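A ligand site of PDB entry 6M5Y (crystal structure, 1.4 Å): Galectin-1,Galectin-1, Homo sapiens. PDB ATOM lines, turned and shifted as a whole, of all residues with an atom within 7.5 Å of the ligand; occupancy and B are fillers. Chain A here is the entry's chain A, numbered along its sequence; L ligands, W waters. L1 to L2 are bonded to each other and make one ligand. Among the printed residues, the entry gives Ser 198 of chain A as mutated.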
ATOM      1  N   SER A 167      36.532  19.506   1.561  1.00  0.00           N
ATOM      2  CA  SER A 167      35.616  19.288   0.441  1.00  0.00           C
ATOM      3  C   SER A 167      35.624  17.838   0.049  1.00  0.00           C
ATOM      4  O   SER A 167      36.660  17.188   0.115  1.00  0.00           O
ATOM      5  CB  SER A 167      36.087  20.128  -0.750  1.00  0.00           C
ATOM      6  OG  SER A 167      35.337  19.834  -1.906  1.00  0.00           O
ATOM      7  N   VAL A 169      33.579  15.160  -3.184  1.00  0.00           N
ATOM      8  CA  VAL A 169      32.762  15.149  -4.401  1.00  0.00           C
ATOM      9  C   VAL A 169      32.350  13.787  -4.746  1.00  0.00           C
ATOM     10  O   VAL A 169      33.147  12.852  -4.697  1.00  0.00           O
ATOM     11  CB  VAL A 169      33.544  15.842  -5.613  1.00  0.00           C
ATOM     12  CG1 VAL A 169      32.820  15.668  -6.922  1.00  0.00           C
ATOM     13  CG2 VAL A 169      33.884  17.318  -5.396  1.00  0.00           C
ATOM     14  N   ASN A 171      30.600  12.488  -8.250  1.00  0.00           N
ATOM     15  CA  ASN A 171      30.196  12.833  -9.618  1.00  0.00           C
ATOM     16  C   ASN A 171      29.502  11.659 -10.235  1.00  0.00           C
ATOM     17  O   ASN A 171      30.017  10.515 -10.172  1.00  0.00           O
ATOM     18  CB  ASN A 171      31.407  13.196 -10.454  1.00  0.00           C
ATOM     19  CG  ASN A 171      31.981  14.569 -10.156  1.00  0.00           C
ATOM     20  OD1 ASN A 171      31.274  15.488  -9.718  1.00  0.00           O
ATOM     21  ND2 ASN A 171      33.252  14.723 -10.431  1.00  0.00           N
ATOM     22  N   HIS A 182      26.984  16.606 -10.033  1.00  0.00           N
ATOM     23  CA  HIS A 182      28.198  16.911  -9.277  1.00  0.00           C
ATOM     24  C   HIS A 182      27.741  17.294  -7.912  1.00  0.00           C
ATOM     25  O   HIS A 182      26.951  18.232  -7.791  1.00  0.00           O
ATOM     26  CB  HIS A 182      28.900  18.053  -9.922  1.00  0.00           C
ATOM     27  CG  HIS A 182      30.009  18.669  -9.135  1.00  0.00           C
ATOM     28  ND1 HIS A 182      31.233  18.080  -8.959  1.00  0.00           N
ATOM     29  CD2 HIS A 182      30.023  19.794  -8.420  1.00  0.00           C
ATOM     30  CE1 HIS A 182      32.016  18.919  -8.322  1.00  0.00           C
ATOM     31  NE2 HIS A 182      31.277  19.919  -7.913  1.00  0.00           N
ATOM     32  N   PHE A 183      28.048  16.459  -6.913  1.00  0.00           N
ATOM     33  CA  PHE A 183      27.530  16.606  -5.542  1.00  0.00           C
ATOM     34  C   PHE A 183      28.730  16.902  -4.655  1.00  0.00           C
ATOM     35  O   PHE A 183      29.615  16.042  -4.571  1.00  0.00           O
ATOM     36  CB  PHE A 183      26.891  15.332  -5.068  1.00  0.00           C
ATOM     37  CG  PHE A 183      26.547  15.320  -3.592  1.00  0.00           C
ATOM     38  CD1 PHE A 183      25.458  16.026  -3.125  1.00  0.00           C
ATOM     39  CD2 PHE A 183      27.333  14.595  -2.695  1.00  0.00           C
ATOM     40  CE1 PHE A 183      25.131  16.009  -1.800  1.00  0.00           C
ATOM     41  CE2 PHE A 183      27.023  14.604  -1.341  1.00  0.00           C
ATOM     42  CZ  PHE A 183      25.953  15.320  -0.885  1.00  0.00           C
ATOM     43  N   ASN A 184      28.755  18.064  -4.030  1.00  0.00           N
ATOM     44  CA  ASN A 184      29.985  18.711  -3.479  1.00  0.00           C
ATOM     45  C   ASN A 184      29.737  19.338  -2.146  1.00  0.00           C
ATOM     46  O   ASN A 184      29.595  20.565  -2.046  1.00  0.00           O
ATOM     47  CB  ASN A 184      30.605  19.712  -4.479  1.00  0.00           C
ATOM     48  CG  ASN A 184      31.945  20.295  -4.022  1.00  0.00           C
ATOM     49  OD1 ASN A 184      32.322  21.284  -4.531  1.00  0.00           O
ATOM     50  ND2 ASN A 184      32.681  19.639  -3.094  1.00  0.00           N
ATOM     51  N   ARG A 186      30.951  21.176   0.843  1.00  0.00           N
ATOM     52  CA  ARG A 186      32.074  22.132   1.053  1.00  0.00           C
ATOM     53  C   ARG A 186      32.028  22.440   2.543  1.00  0.00           C
ATOM     54  O   ARG A 186      31.153  23.196   3.020  1.00  0.00           O
ATOM     55  CB  ARG A 186      31.990  23.403   0.200  1.00  0.00           C
ATOM     56  CG  ARG A 186      32.081  23.090  -1.271  1.00  0.00           C
ATOM     57  CD  ARG A 186      31.858  24.296  -2.118  1.00  0.00           C
ATOM     58  NE  ARG A 186      31.863  23.995  -3.546  1.00  0.00           N
ATOM     59  CZ  ARG A 186      31.746  24.898  -4.514  1.00  0.00           C
ATOM     60  NH1 ARG A 186      31.738  24.479  -5.789  1.00  0.00           N
ATOM     61  NH2 ARG A 186      31.589  26.202  -4.244  1.00  0.00           N
ATOM     62  N   ALA A 189      35.651  25.467   1.441  1.00  0.00           N
ATOM     63  CA  ALA A 189      36.235  25.384   0.077  1.00  0.00           C
ATOM     64  C   ALA A 189      35.572  26.385  -0.869  1.00  0.00           C
ATOM     65  O   ALA A 189      34.350  26.550  -0.810  1.00  0.00           O
ATOM     66  CB  ALA A 189      36.075  23.978  -0.459  1.00  0.00           C
ATOM     67  N   HIS A 190      36.392  27.081  -1.683  1.00  0.00           N
ATOM     68  CA  HIS A 190      35.905  28.060  -2.687  1.00  0.00           C
ATOM     69  C   HIS A 190      35.113  29.202  -2.018  1.00  0.00           C
ATOM     70  O   HIS A 190      34.146  29.711  -2.604  1.00  0.00           O
ATOM     71  CB  HIS A 190      35.048  27.349  -3.753  1.00  0.00           C
ATOM     72  CG  HIS A 190      35.660  26.092  -4.293  1.00  0.00           C
ATOM     73  ND1 HIS A 190      36.802  26.095  -5.061  1.00  0.00           N
ATOM     74  CD2 HIS A 190      35.283  24.798  -4.170  1.00  0.00           C
ATOM     75  CE1 HIS A 190      37.118  24.852  -5.379  1.00  0.00           C
ATOM     76  NE2 HIS A 190      36.213  24.044  -4.860  1.00  0.00           N
ATOM     77  N   ASP A 192      33.042  28.838   0.426  1.00  0.00           N
ATOM     78  CA  ASP A 192      31.829  28.337   1.074  1.00  0.00           C
ATOM     79  C   ASP A 192      32.234  27.602   2.317  1.00  0.00           C
ATOM     80  O   ASP A 192      33.201  26.816   2.307  1.00  0.00           O
ATOM     81  CB  ASP A 192      31.077  27.359   0.187  1.00  0.00           C
ATOM     82  CG  ASP A 192      30.348  28.037  -0.952  1.00  0.00           C
ATOM     83  OD1 ASP A 192      29.354  28.768  -0.680  1.00  0.00           O
ATOM     84  OD2 ASP A 192      30.752  27.781  -2.117  1.00  0.00           O
ATOM     85  N   VAL A 197      26.967  22.068  -2.376  1.00  0.00           N
ATOM     86  CA  VAL A 197      26.788  22.588  -3.736  1.00  0.00           C
ATOM     87  C   VAL A 197      26.575  21.430  -4.683  1.00  0.00           C
ATOM     88  O   VAL A 197      27.370  20.494  -4.674  1.00  0.00           O
ATOM     89  CB  VAL A 197      28.007  23.431  -4.158  1.00  0.00           C
ATOM     90  CG1 VAL A 197      27.885  23.898  -5.601  1.00  0.00           C
ATOM     91  CG2 VAL A 197      28.305  24.570  -3.184  1.00  0.00           C
ATOM     92  N   SER A 198      25.529  21.526  -5.512  1.00  0.00           N
ATOM     93  CA  SER A 198      25.251  20.527  -6.568  1.00  0.00           C
ATOM     94  C   SER A 198      25.207  21.234  -7.927  1.00  0.00           C
ATOM     95  O   SER A 198      24.852  22.403  -8.007  1.00  0.00           O
ATOM     96  CB  SER A 198      23.982  19.746  -6.335  1.00  0.00           C
ATOM     97  OG  SER A 198      24.011  19.007  -5.125  1.00  0.00           O
ATOM     98  N   ASN A 199      25.628  20.528  -8.966  1.00  0.00           N
ATOM     99  CA  ASN A 199      25.577  21.096 -10.303  1.00  0.00           C
ATOM    100  C   ASN A 199      25.501  19.987 -11.336  1.00  0.00           C
ATOM    101  O   ASN A 199      25.716  18.812 -11.020  1.00  0.00           O
ATOM    102  CB  ASN A 199      26.798  21.990 -10.605  1.00  0.00           C
ATOM    103  CG  ASN A 199      26.446  23.134 -11.566  1.00  0.00           C
ATOM    104  OD1 ASN A 199      25.397  23.107 -12.223  1.00  0.00           O
ATOM    105  ND2 ASN A 199      27.282  24.161 -11.635  1.00  0.00           N
ATOM    106  N   SER A 200      25.158  20.381 -12.568  1.00  0.00           N
ATOM    107  CA  SER A 200      25.315  19.556 -13.735  1.00  0.00           C
ATOM    108  C   SER A 200      26.577  19.973 -14.484  1.00  0.00           C
ATOM    109  O   SER A 200      27.115  21.078 -14.270  1.00  0.00           O
ATOM    110  CB  SER A 200      24.095  19.681 -14.637  1.00  0.00           C
ATOM    111  OG  SER A 200      23.835  21.056 -14.904  1.00  0.00           O
ATOM    112  N   LYS A 201      27.059  19.078 -15.333  1.00  0.00           N
ATOM    113  CA  LYS A 201      28.118  19.418 -16.283  1.00  0.00           C
ATOM    114  C   LYS A 201      27.766  18.828 -17.622  1.00  0.00           C
ATOM    115  O   LYS A 201      27.455  17.626 -17.723  1.00  0.00           O
ATOM    116  CB  LYS A 201      29.487  18.924 -15.823  1.00  0.00           C
ATOM    117  CG  LYS A 201      30.650  19.429 -16.599  1.00  0.00           C
ATOM    118  CD  LYS A 201      31.964  18.867 -16.076  1.00  0.00           C
ATOM    119  CE  LYS A 201      32.873  19.939 -15.618  1.00  0.00           C
ATOM    120  NZ  LYS A 201      34.176  19.317 -15.264  1.00  0.00           N
ATOM    121  N   TRP A 206      29.850  23.689 -16.751  1.00  0.00           N
ATOM    122  CA  TRP A 206      29.066  23.731 -15.527  1.00  0.00           C
ATOM    123  C   TRP A 206      27.710  24.394 -15.749  1.00  0.00           C
ATOM    124  O   TRP A 206      27.644  25.395 -16.430  1.00  0.00           O
ATOM    125  CB  TRP A 206      29.785  24.465 -14.386  1.00  0.00           C
ATOM    126  CG  TRP A 206      30.987  23.772 -13.877  1.00  0.00           C
ATOM    127  CD1 TRP A 206      32.247  24.257 -13.865  1.00  0.00           C
ATOM    128  CD2 TRP A 206      31.030  22.522 -13.212  1.00  0.00           C
ATOM    129  NE1 TRP A 206      33.089  23.362 -13.259  1.00  0.00           N
ATOM    130  CE2 TRP A 206      32.365  22.273 -12.884  1.00  0.00           C
ATOM    131  CE3 TRP A 206      30.077  21.545 -12.919  1.00  0.00           C
ATOM    132  CZ2 TRP A 206      32.777  21.089 -12.245  1.00  0.00           C
ATOM    133  CZ3 TRP A 206      30.471  20.336 -12.299  1.00  0.00           C
ATOM    134  CH2 TRP A 206      31.822  20.112 -12.002  1.00  0.00           C
ATOM    135  N   GLY A 207      26.675  23.820 -15.158  1.00  0.00           N
ATOM    136  CA  GLY A 207      25.324  24.392 -15.169  1.00  0.00           C
ATOM    137  C   GLY A 207      25.155  25.401 -14.074  1.00  0.00           C
ATOM    138  O   GLY A 207      26.146  25.943 -13.532  1.00  0.00           O
ATOM    139  N   THR A 208      23.908  25.620 -13.694  1.00  0.00           N
ATOM    140  CA  THR A 208      23.583  26.541 -12.612  1.00  0.00           C
ATOM    141  C   THR A 208      23.567  25.764 -11.290  1.00  0.00           C
ATOM    142  O   THR A 208      22.854  24.741 -11.167  1.00  0.00           O
ATOM    143  CB  THR A 208      22.247  27.237 -12.865  1.00  0.00           C
ATOM    144  OG1 THR A 208      22.392  28.054 -14.033  1.00  0.00           O
ATOM    145  CG2 THR A 208      21.849  28.114 -11.669  1.00  0.00           C
ATOM    146  N   GLU A 209      24.329  26.247 -10.307  1.00  0.00           N
ATOM    147  CA  GLU A 209      24.456  25.543  -9.022  1.00  0.00           C
ATOM    148  C   GLU A 209      23.161  25.545  -8.257  1.00  0.00           C
ATOM    149  O   GLU A 209      22.304  26.417  -8.473  1.00  0.00           O
ATOM    150  CB  GLU A 209      25.557  26.144  -8.155  1.00  0.00           C
ATOM    151  CG  GLU A 209      26.955  25.925  -8.731  1.00  0.00           C
ATOM    152  CD  GLU A 209      28.064  26.614  -7.935  1.00  0.00           C
ATOM    153  OE1 GLU A 209      27.740  27.476  -7.112  1.00  0.00           O
ATOM    154  OE2 GLU A 209      29.245  26.303  -8.121  1.00  0.00           O
ATOM    155  N   GLN A 210      22.986  24.517  -7.436  1.00  0.00           N
ATOM    156  CA  GLN A 210      21.948  24.479  -6.421  1.00  0.00           C
ATOM    157  C   GLN A 210      22.603  24.242  -5.104  1.00  0.00           C
ATOM    158  O   GLN A 210      23.377  23.302  -4.964  1.00  0.00           O
ATOM    159  CB  GLN A 210      21.019  23.331  -6.697  1.00  0.00           C
ATOM    160  CG  GLN A 210      19.850  23.186  -5.716  1.00  0.00           C
ATOM    161  CD  GLN A 210      18.932  22.040  -6.063  1.00  0.00           C
ATOM    162  OE1 GLN A 210      18.325  22.013  -7.168  1.00  0.00           O
ATOM    163  NE2 GLN A 210      18.800  21.108  -5.145  1.00  0.00           N
ATOM    164  N   ARG A 211      22.260  25.050  -4.129  1.00  0.00           N
ATOM    165  CA  ARG A 211      22.865  24.954  -2.802  1.00  0.00           C
ATOM    166  C   ARG A 211      21.811  24.565  -1.812  1.00  0.00           C
ATOM    167  O   ARG A 211      20.693  25.039  -1.921  1.00  0.00           O
ATOM    168  CB  ARG A 211      23.481  26.277  -2.444  1.00  0.00           C
ATOM    169  CG  ARG A 211      24.775  26.485  -3.102  1.00  0.00           C
ATOM    170  CD  ARG A 211      25.284  27.844  -2.700  1.00  0.00           C
ATOM    171  NE  ARG A 211      26.706  28.043  -2.932  1.00  0.00           N
ATOM    172  CZ  ARG A 211      27.248  28.140  -4.117  1.00  0.00           C
ATOM    173  NH1 ARG A 211      28.575  28.407  -4.246  1.00  0.00           N
ATOM    174  NH2 ARG A 211      26.486  28.097  -5.206  1.00  0.00           N
ATOM    175  N   ASP A 261      36.041  12.026  -5.228  1.00  0.00           N
ATOM    176  CA  ASP A 261      37.318  12.574  -4.868  1.00  0.00           C
ATOM    177  C   ASP A 261      37.205  13.408  -3.633  1.00  0.00           C
ATOM    178  O   ASP A 261      36.155  13.890  -3.295  1.00  0.00           O
ATOM    179  CB  ASP A 261      37.970  13.378  -6.047  1.00  0.00           C
ATOM    180  CG  ASP A 261      37.313  14.752  -6.307  1.00  0.00           C
ATOM    181  OD1 ASP A 261      36.370  14.782  -7.099  1.00  0.00           O
ATOM    182  OD2 ASP A 261      37.800  15.819  -5.801  1.00  0.00           O
HETATM  183  C1  LIG L   1      31.630  30.526  -8.575  1.00  0.00           C
HETATM  184  C2  LIG L   1      30.838  29.476  -7.768  1.00  0.00           C
HETATM  185  C3  LIG L   1      31.681  28.284  -7.357  1.00  0.00           C
HETATM  186  C4  LIG L   1      32.467  27.773  -8.565  1.00  0.00           C
HETATM  187  C5  LIG L   1      33.276  28.879  -9.224  1.00  0.00           C
HETATM  188  C6  LIG L   1      34.001  28.406 -10.499  1.00  0.00           C
HETATM  189  O1  LIG L   1      32.502  31.326  -7.761  1.00  0.00           O
HETATM  190  O2  LIG L   1      30.376  30.131  -6.586  1.00  0.00           O
HETATM  191  O3  LIG L   1      30.984  27.295  -6.735  1.00  0.00           O
HETATM  192  O4  LIG L   1      33.344  26.755  -8.058  1.00  0.00           O
HETATM  193  O5  LIG L   1      32.415  29.951  -9.612  1.00  0.00           O
HETATM  194  O6  LIG L   1      33.056  27.771 -11.412  1.00  0.00           O
HETATM  195  C1  LG2 L   2      33.314  25.555  -8.822  1.00  0.00           C
HETATM  196  C2  LG2 L   2      34.421  24.648  -8.326  1.00  0.00           C
HETATM  197  C3  LG2 L   2      34.212  23.247  -8.980  1.00  0.00           C
HETATM  198  C4  LG2 L   2      32.804  22.639  -8.833  1.00  0.00           C
HETATM  199  C5  LG2 L   2      31.847  23.721  -9.368  1.00  0.00           C
HETATM  200  C6  LG2 L   2      30.408  23.359  -9.283  1.00  0.00           C
HETATM  201  O1  LG2 L   2      35.667  25.180  -8.585  1.00  0.00           O
HETATM  202  O2  LG2 L   2      35.191  22.307  -8.438  1.00  0.00           O
HETATM  203  O3  LG2 L   2      32.529  22.374  -7.437  1.00  0.00           O
HETATM  204  O4  LG2 L   2      32.057  24.920  -8.631  1.00  0.00           O
HETATM  205  O5  LG2 L   2      29.560  24.405  -9.801  1.00  0.00           O
HETATM  206  O   HOH W   1      31.441  29.830  -3.974  1.00  0.00           O
HETATM  207  O   HOH W   2      36.576  27.459  -7.702  1.00  0.00           O
HETATM  208  O   HOH W   3      34.860  21.654  -5.683  1.00  0.00           O
HETATM  209  O   HOH W   4      30.502  26.571 -11.450  1.00  0.00           O
HETATM  210  O   HOH W   5      35.270  19.729  -9.409  1.00  0.00           O
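The side-chain carboxylate of Glu 209 lies within hydrogen-bond range of an oxygen (O3) of LIG L1.
NH2 of Arg 186 sits at hydrogen-bond distance from O3 of LIG L1, at 2.8 Å.
NE2 of His 182 sits at hydrogen-bond distance from O3 of LG2 L2.
ND2 of Asn 199 is in hydrogen-bond range of O5 of LG2 L2 (2.9 Å).
OD1 of Asn 184 lies within hydrogen-bond range of O3 of LG2 L2 (3.1 Å).
An oxygen (O2) of LIG L1 sits at hydrogen-bond distance from the guanidinium group (NH1) of Arg 211.
OE2 of Glu 209 is in salt-bridge range of NH1 of Arg 186 (3.9 Å).
The guanidinium group of Arg 186 is in hydrogen-bond range of the side-chain amide oxygen of Asn 184 (2.9 Å).
The guanidinium group (NH2) of Arg 186 is in salt-bridge range of the side-chain carboxylate (OD2) of Asp 192 (2.8 Å).
The backbone carbonyl oxygen (O) of Asn 199 is in hydrogen-bond range of the backbone NH (N) of His 182, at 2.7 Å.
The side-chain amide nitrogen (ND2) of Asn 199 lies within hydrogen-bond range of the backbone carbonyl oxygen (O) of Gly 207.
OD1 of Asn 199 sits close to O of Thr 208.
The side-chain amide nitrogen (ND2) of Asn 184 is in hydrogen-bond range of the side-chain hydroxyl (OG) of Ser 167 (2.9 Å).
The guanidinium group (NH1) of Arg 211 is in salt-bridge range of the side-chain carboxylate (OD2) of Asp 192.
Residues that only touch the ligand: His 190 (3.5 Å) and Trp 206 (3.7 Å).
Hydrophobic or aromatic side chains within 4 Å of the ligand: His 182, His 190 and Trp 206.
Within 4 Å of the ligand: His 182, Asn 184, Arg 186, His 190, Asn 199, Trp 206, Glu 209 and Arg 211.
The nearest printed residue that does not touch the ligand is Val 197 (4.5 Å).
Water W2 lies within hydrogen-bond range of an oxygen (O1) of LG2 L2 (2.6 Å) and a ring nitrogen (ND1) of His 190 (3.0 Å).
Water W1 lies within hydrogen-bond range of O2 of LIG L1 (2.8 Å), OD2 of Asp 192 (2.8 Å), O of His 190 (3.0 Å) and NH1 of Arg 211 (3.2 Å).
Water W3 lies within hydrogen-bond range of OD1 of Asn 184 (2.8 Å), O2 of LG2 L2 (2.9 Å) and NE2 of His 190 (2.9 Å).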
